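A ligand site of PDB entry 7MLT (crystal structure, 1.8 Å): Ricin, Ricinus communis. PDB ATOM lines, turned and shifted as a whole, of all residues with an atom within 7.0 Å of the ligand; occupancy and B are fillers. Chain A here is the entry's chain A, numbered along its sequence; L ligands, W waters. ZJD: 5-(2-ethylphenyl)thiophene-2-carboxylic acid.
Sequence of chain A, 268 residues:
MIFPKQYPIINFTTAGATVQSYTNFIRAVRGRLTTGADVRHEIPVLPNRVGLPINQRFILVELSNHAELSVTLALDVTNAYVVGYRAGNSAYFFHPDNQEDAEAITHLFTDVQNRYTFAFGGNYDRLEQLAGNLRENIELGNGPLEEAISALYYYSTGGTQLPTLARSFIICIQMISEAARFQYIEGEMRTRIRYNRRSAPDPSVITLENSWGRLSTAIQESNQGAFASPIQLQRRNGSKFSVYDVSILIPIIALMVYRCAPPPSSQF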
ATOM      1  N   TYR A 184       4.665  29.931 -23.059  1.00  0.00           N
ATOM      2  CA  TYR A 184       5.027  30.083 -21.636  1.00  0.00           C
ATOM      3  C   TYR A 184       4.442  31.402 -21.109  1.00  0.00           C
ATOM      4  O   TYR A 184       3.864  31.416 -20.014  1.00  0.00           O
ATOM      5  CB  TYR A 184       6.541  30.026 -21.453  1.00  0.00           C
ATOM      6  CG  TYR A 184       6.995  30.135 -20.024  1.00  0.00           C
ATOM      7  CD1 TYR A 184       6.862  29.053 -19.166  1.00  0.00           C
ATOM      8  CD2 TYR A 184       7.548  31.303 -19.524  1.00  0.00           C
ATOM      9  CE1 TYR A 184       7.258  29.137 -17.845  1.00  0.00           C
ATOM     10  CE2 TYR A 184       7.957  31.395 -18.216  1.00  0.00           C
ATOM     11  CZ  TYR A 184       7.800  30.321 -17.361  1.00  0.00           C
ATOM     12  OH  TYR A 184       8.199  30.382 -16.063  1.00  0.00           O
ATOM     13  N   GLU A 188       1.403  32.341 -18.385  1.00  0.00           N
ATOM     14  CA  GLU A 188       1.626  33.323 -17.286  1.00  0.00           C
ATOM     15  C   GLU A 188       0.451  34.311 -17.230  1.00  0.00           C
ATOM     16  O   GLU A 188       0.033  34.657 -16.107  1.00  0.00           O
ATOM     17  CB  GLU A 188       2.954  34.048 -17.490  1.00  0.00           C
ATOM     18  CG  GLU A 188       4.155  33.205 -17.156  1.00  0.00           C
ATOM     19  CD  GLU A 188       4.496  33.125 -15.688  1.00  0.00           C
ATOM     20  OE1 GLU A 188       4.164  34.074 -14.920  1.00  0.00           O
ATOM     21  OE2 GLU A 188       5.081  32.110 -15.306  1.00  0.00           O
ATOM     22  N   ASP A 202       8.285  37.551 -13.636  1.00  0.00           N
ATOM     23  CA  ASP A 202       9.487  37.071 -12.904  1.00  0.00           C
ATOM     24  C   ASP A 202      10.648  36.926 -13.891  1.00  0.00           C
ATOM     25  O   ASP A 202      10.483  37.107 -15.094  1.00  0.00           O
ATOM     26  CB  ASP A 202       9.131  35.836 -12.090  1.00  0.00           C
ATOM     27  CG  ASP A 202       8.921  34.573 -12.895  1.00  0.00           C
ATOM     28  OD1 ASP A 202       9.506  34.462 -13.985  1.00  0.00           O
ATOM     29  OD2 ASP A 202       8.181  33.688 -12.406  1.00  0.00           O
ATOM     30  N   SER A 204      12.165  34.451 -15.254  1.00  0.00           N
ATOM     31  CA  SER A 204      11.963  33.430 -16.324  1.00  0.00           C
ATOM     32  C   SER A 204      11.257  34.080 -17.512  1.00  0.00           C
ATOM     33  O   SER A 204      11.672  33.843 -18.673  1.00  0.00           O
ATOM     34  CB  SER A 204      11.223  32.219 -15.816  1.00  0.00           C
ATOM     35  OG  SER A 204       9.857  32.487 -15.569  1.00  0.00           O
ATOM     36  N   VAL A 205      10.278  34.935 -17.243  1.00  0.00           N
ATOM     37  CA  VAL A 205       9.491  35.638 -18.308  1.00  0.00           C
ATOM     38  C   VAL A 205      10.407  36.684 -18.948  1.00  0.00           C
ATOM     39  O   VAL A 205      10.467  36.734 -20.180  1.00  0.00           O
ATOM     40  CB  VAL A 205       8.199  36.242 -17.740  1.00  0.00           C
ATOM     41  CG1 VAL A 205       7.495  37.127 -18.745  1.00  0.00           C
ATOM     42  CG2 VAL A 205       7.254  35.152 -17.231  1.00  0.00           C
ATOM     43  N   LEU A 208      13.215  35.181 -21.089  1.00  0.00           N
ATOM     44  CA  LEU A 208      12.609  34.613 -22.326  1.00  0.00           C
ATOM     45  C   LEU A 208      12.351  35.729 -23.336  1.00  0.00           C
ATOM     46  O   LEU A 208      12.785  35.607 -24.483  1.00  0.00           O
ATOM     47  CB  LEU A 208      11.327  33.875 -21.944  1.00  0.00           C
ATOM     48  CG  LEU A 208      10.841  32.820 -22.930  1.00  0.00           C
ATOM     49  CD1 LEU A 208      11.907  31.767 -23.213  1.00  0.00           C
ATOM     50  CD2 LEU A 208       9.584  32.168 -22.386  1.00  0.00           C
ATOM     51  N   LEU A 233      18.986  30.503 -20.171  1.00  0.00           N
ATOM     52  CA  LEU A 233      17.674  31.052 -19.731  1.00  0.00           C
ATOM     53  C   LEU A 233      17.665  31.086 -18.199  1.00  0.00           C
ATOM     54  O   LEU A 233      18.630  30.627 -17.587  1.00  0.00           O
ATOM     55  CB  LEU A 233      16.537  30.185 -20.275  1.00  0.00           C
ATOM     56  CG  LEU A 233      16.387  30.166 -21.786  1.00  0.00           C
ATOM     57  CD1 LEU A 233      15.240  29.267 -22.212  1.00  0.00           C
ATOM     58  CD2 LEU A 233      16.194  31.572 -22.347  1.00  0.00           C
ATOM     59  N   GLN A 234      16.596  31.632 -17.627  1.00  0.00           N
ATOM     60  CA  GLN A 234      16.461  31.777 -16.158  1.00  0.00           C
ATOM     61  C   GLN A 234      15.220  31.035 -15.684  1.00  0.00           C
ATOM     62  O   GLN A 234      14.200  31.019 -16.397  1.00  0.00           O
ATOM     63  CB  GLN A 234      16.396  33.256 -15.771  1.00  0.00           C
ATOM     64  CG  GLN A 234      17.768  33.905 -15.615  1.00  0.00           C
ATOM     65  CD  GLN A 234      17.637  35.308 -15.067  1.00  0.00           C
ATOM     66  OE1 GLN A 234      17.898  35.576 -13.895  1.00  0.00           O
ATOM     67  NE2 GLN A 234      17.196  36.214 -15.912  1.00  0.00           N
ATOM     68  N   ARG A 235      15.339  30.429 -14.506  1.00  0.00           N
ATOM     69  CA  ARG A 235      14.213  29.896 -13.704  1.00  0.00           C
ATOM     70  C   ARG A 235      13.481  31.054 -13.013  1.00  0.00           C
ATOM     71  O   ARG A 235      13.996  32.188 -13.075  1.00  0.00           O
ATOM     72  CB  ARG A 235      14.753  28.913 -12.662  1.00  0.00           C
ATOM     73  CG  ARG A 235      15.475  27.710 -13.255  1.00  0.00           C
ATOM     74  CD  ARG A 235      15.614  26.574 -12.262  1.00  0.00           C
ATOM     75  NE  ARG A 235      16.203  25.393 -12.879  1.00  0.00           N
ATOM     76  CZ  ARG A 235      17.502  25.206 -13.077  1.00  0.00           C
ATOM     77  NH1 ARG A 235      18.369  26.139 -12.701  1.00  0.00           N
ATOM     78  NH2 ARG A 235      17.938  24.098 -13.654  1.00  0.00           N
ATOM     79  N   ARG A 236      12.361  30.757 -12.366  1.00  0.00           N
ATOM     80  CA  ARG A 236      11.542  31.755 -11.615  1.00  0.00           C
ATOM     81  C   ARG A 236      12.395  32.434 -10.545  1.00  0.00           C
ATOM     82  O   ARG A 236      12.178  33.631 -10.326  1.00  0.00           O
ATOM     83  CB  ARG A 236      10.342  31.091 -10.954  1.00  0.00           C
ATOM     84  CG  ARG A 236       9.314  30.598 -11.953  1.00  0.00           C
ATOM     85  CD  ARG A 236       7.986  30.251 -11.331  1.00  0.00           C
ATOM     86  NE  ARG A 236       7.211  29.661 -12.417  1.00  0.00           N
ATOM     87  CZ  ARG A 236       6.562  30.353 -13.336  1.00  0.00           C
ATOM     88  NH1 ARG A 236       6.532  31.681 -13.302  1.00  0.00           N
ATOM     89  NH2 ARG A 236       5.930  29.709 -14.304  1.00  0.00           N
ATOM     90  N   ASN A 237      13.341  31.715  -9.927  1.00  0.00           N
ATOM     91  CA  ASN A 237      14.152  32.227  -8.788  1.00  0.00           C
ATOM     92  C   ASN A 237      15.391  32.965  -9.308  1.00  0.00           C
ATOM     93  O   ASN A 237      16.177  33.442  -8.478  1.00  0.00           O
ATOM     94  CB  ASN A 237      14.510  31.097  -7.823  1.00  0.00           C
ATOM     95  CG  ASN A 237      15.397  30.033  -8.415  1.00  0.00           C
ATOM     96  OD1 ASN A 237      15.882  30.157  -9.544  1.00  0.00           O
ATOM     97  ND2 ASN A 237      15.628  28.970  -7.661  1.00  0.00           N
ATOM     98  N   GLY A 238      15.553  33.073 -10.636  1.00  0.00           N
ATOM     99  CA  GLY A 238      16.634  33.821 -11.279  1.00  0.00           C
ATOM    100  C   GLY A 238      17.856  32.964 -11.573  1.00  0.00           C
ATOM    101  O   GLY A 238      18.772  33.459 -12.255  1.00  0.00           O
ATOM    102  N   SER A 239      17.887  31.712 -11.088  1.00  0.00           N
ATOM    103  CA  SER A 239      19.004  30.756 -11.322  1.00  0.00           C
ATOM    104  C   SER A 239      19.108  30.480 -12.824  1.00  0.00           C
ATOM    105  O   SER A 239      18.041  30.356 -13.487  1.00  0.00           O
ATOM    106  CB  SER A 239      18.846  29.486 -10.517  1.00  0.00           C
ATOM    107  OG  SER A 239      17.684  28.750 -10.895  1.00  0.00           O
ATOM    108  N   PHE A 241      20.326  28.388 -16.329  1.00  0.00           N
ATOM    109  CA  PHE A 241      20.503  27.018 -16.864  1.00  0.00           C
ATOM    110  C   PHE A 241      20.695  27.107 -18.372  1.00  0.00           C
ATOM    111  O   PHE A 241      20.240  28.090 -18.981  1.00  0.00           O
ATOM    112  CB  PHE A 241      19.343  26.091 -16.474  1.00  0.00           C
ATOM    113  CG  PHE A 241      18.034  26.391 -17.158  1.00  0.00           C
ATOM    114  CD1 PHE A 241      17.150  27.317 -16.628  1.00  0.00           C
ATOM    115  CD2 PHE A 241      17.682  25.725 -18.326  1.00  0.00           C
ATOM    116  CE1 PHE A 241      15.949  27.581 -17.260  1.00  0.00           C
ATOM    117  CE2 PHE A 241      16.479  25.998 -18.955  1.00  0.00           C
ATOM    118  CZ  PHE A 241      15.610  26.922 -18.412  1.00  0.00           C
ATOM    119  N   VAL A 243      20.440  25.717 -22.367  1.00  0.00           N
ATOM    120  CA  VAL A 243      19.656  24.967 -23.393  1.00  0.00           C
ATOM    121  C   VAL A 243      20.608  24.681 -24.548  1.00  0.00           C
ATOM    122  O   VAL A 243      21.226  25.646 -25.066  1.00  0.00           O
ATOM    123  CB  VAL A 243      18.414  25.760 -23.845  1.00  0.00           C
ATOM    124  CG1 VAL A 243      17.593  24.976 -24.848  1.00  0.00           C
ATOM    125  CG2 VAL A 243      17.557  26.188 -22.666  1.00  0.00           C
ATOM    126  N   ILE A 248      13.538  20.963 -25.854  1.00  0.00           N
ATOM    127  CA  ILE A 248      12.842  21.513 -24.658  1.00  0.00           C
ATOM    128  C   ILE A 248      12.055  22.787 -25.032  1.00  0.00           C
ATOM    129  O   ILE A 248      11.180  23.155 -24.239  1.00  0.00           O
ATOM    130  CB  ILE A 248      13.889  21.724 -23.546  1.00  0.00           C
ATOM    131  CG1 ILE A 248      13.243  21.907 -22.163  1.00  0.00           C
ATOM    132  CG2 ILE A 248      14.850  22.851 -23.879  1.00  0.00           C
ATOM    133  CD1 ILE A 248      14.236  22.096 -21.038  1.00  0.00           C
ATOM    134  N   LEU A 249      12.279  23.401 -26.197  1.00  0.00           N
ATOM    135  CA  LEU A 249      11.746  24.753 -26.547  1.00  0.00           C
ATOM    136  C   LEU A 249      10.472  24.671 -27.377  1.00  0.00           C
ATOM    137  O   LEU A 249       9.773  25.686 -27.463  1.00  0.00           O
ATOM    138  CB  LEU A 249      12.814  25.552 -27.307  1.00  0.00           C
ATOM    139  CG  LEU A 249      14.062  25.897 -26.506  1.00  0.00           C
ATOM    140  CD1 LEU A 249      15.033  26.692 -27.355  1.00  0.00           C
ATOM    141  CD2 LEU A 249      13.701  26.671 -25.247  1.00  0.00           C
ATOM    142  N   ILE A 252       7.440  25.974 -25.730  1.00  0.00           N
ATOM    143  CA  ILE A 252       7.732  27.274 -25.033  1.00  0.00           C
ATOM    144  C   ILE A 252       7.672  28.456 -26.033  1.00  0.00           C
ATOM    145  O   ILE A 252       7.163  29.548 -25.656  1.00  0.00           O
ATOM    146  CB  ILE A 252       9.124  27.178 -24.379  1.00  0.00           C
ATOM    147  CG1 ILE A 252       9.150  26.104 -23.302  1.00  0.00           C
ATOM    148  CG2 ILE A 252       9.603  28.514 -23.839  1.00  0.00           C
ATOM    149  CD1 ILE A 252       8.026  26.198 -22.307  1.00  0.00           C
HETATM  150  C10 ZJD L   1      12.564  27.046 -20.600  1.00  0.00           C
HETATM  151  C13 ZJD L   1      11.163  29.707 -19.672  1.00  0.00           C
HETATM  152  C01 ZJD L   1      10.827  28.180 -14.960  1.00  0.00           C
HETATM  153  C02 ZJD L   1      11.652  27.150 -14.382  1.00  0.00           C
HETATM  154  S03 ZJD L   1      12.330  26.304 -15.531  1.00  0.00           S
HETATM  155  C04 ZJD L   1      11.775  26.947 -16.857  1.00  0.00           C
HETATM  156  C05 ZJD L   1      10.886  28.037 -16.526  1.00  0.00           C
HETATM  157  C06 ZJD L   1      12.058  26.545 -18.299  1.00  0.00           C
HETATM  158  C07 ZJD L   1      12.029  25.189 -18.614  1.00  0.00           C
HETATM  159  C08 ZJD L   1      12.272  24.761 -19.903  1.00  0.00           C
HETATM  160  C09 ZJD L   1      12.551  25.687 -20.902  1.00  0.00           C
HETATM  161  C11 ZJD L   1      12.324  27.505 -19.308  1.00  0.00           C
HETATM  162  C12 ZJD L   1      12.382  29.027 -19.061  1.00  0.00           C
HETATM  163  C14 ZJD L   1      11.812  27.003 -12.882  1.00  0.00           C
HETATM  164  O15 ZJD L   1      11.342  27.877 -12.102  1.00  0.00           O
HETATM  165  O16 ZJD L   1      12.433  26.011 -12.428  1.00  0.00           O
HETATM  166  O   HOH W   1      12.693  28.713  -9.756  1.00  0.00           O
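The backbone NH (N) of Arg 236 is in hydrogen-bond range of an oxygen (O15) of the ligand (3.1 Å).
NE of Arg 235 is in salt-bridge range of O16 of the ligand, 3.8 Å away.
OH of Tyr 184 is in hydrogen-bond range of NH2 of Arg 236 (2.9 Å).
NH1 of Arg 236 is in salt-bridge range of OD2 of Asp 202, 2.7 Å away.
NH1 of Arg 236 is in salt-bridge range of OE2 of Glu 188.
NH1 of Arg 235 lies within hydrogen-bond range of OG of Ser 239.
The backbone carbonyl oxygen of Phe 241 sits at hydrogen-bond distance from the backbone NH of Leu 233, 3.0 Å away.
The side-chain hydroxyl (OH) of Tyr 184 sits at hydrogen-bond distance from the side-chain hydroxyl (OG) of Ser 204, at 2.7 Å.
O of Gly 238 lies close to OE1 of Gln 234, 2.8 Å away.
Merely in contact with the ligand: Tyr 184 (3.6 Å), Leu 208 (3.99 Å), Leu 233 (3.8 Å), Gln 234 (3.8 Å), Phe 241 (3.5 Å) and Ile 248 (3.5 Å).
Hydrophobic or aromatic side chains that line the ligand: Tyr 184, Leu 208, Leu 233, Phe 241 and Ile 248.
Within 4 Å of the ligand: Tyr 184, Leu 208, Leu 233, Gln 234, Arg 235, Arg 236, Phe 241 and Ile 248.
The nearest printed residue that does not touch the ligand is Ser 204 (4.1 Å).
Water W1 lies within hydrogen-bond range of an oxygen (O15) of the ligand (2.8 Å), the backbone NH (N) of Asn 237 (3.1 Å) and the backbone NH (N) of Arg 236 (3.3 Å).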
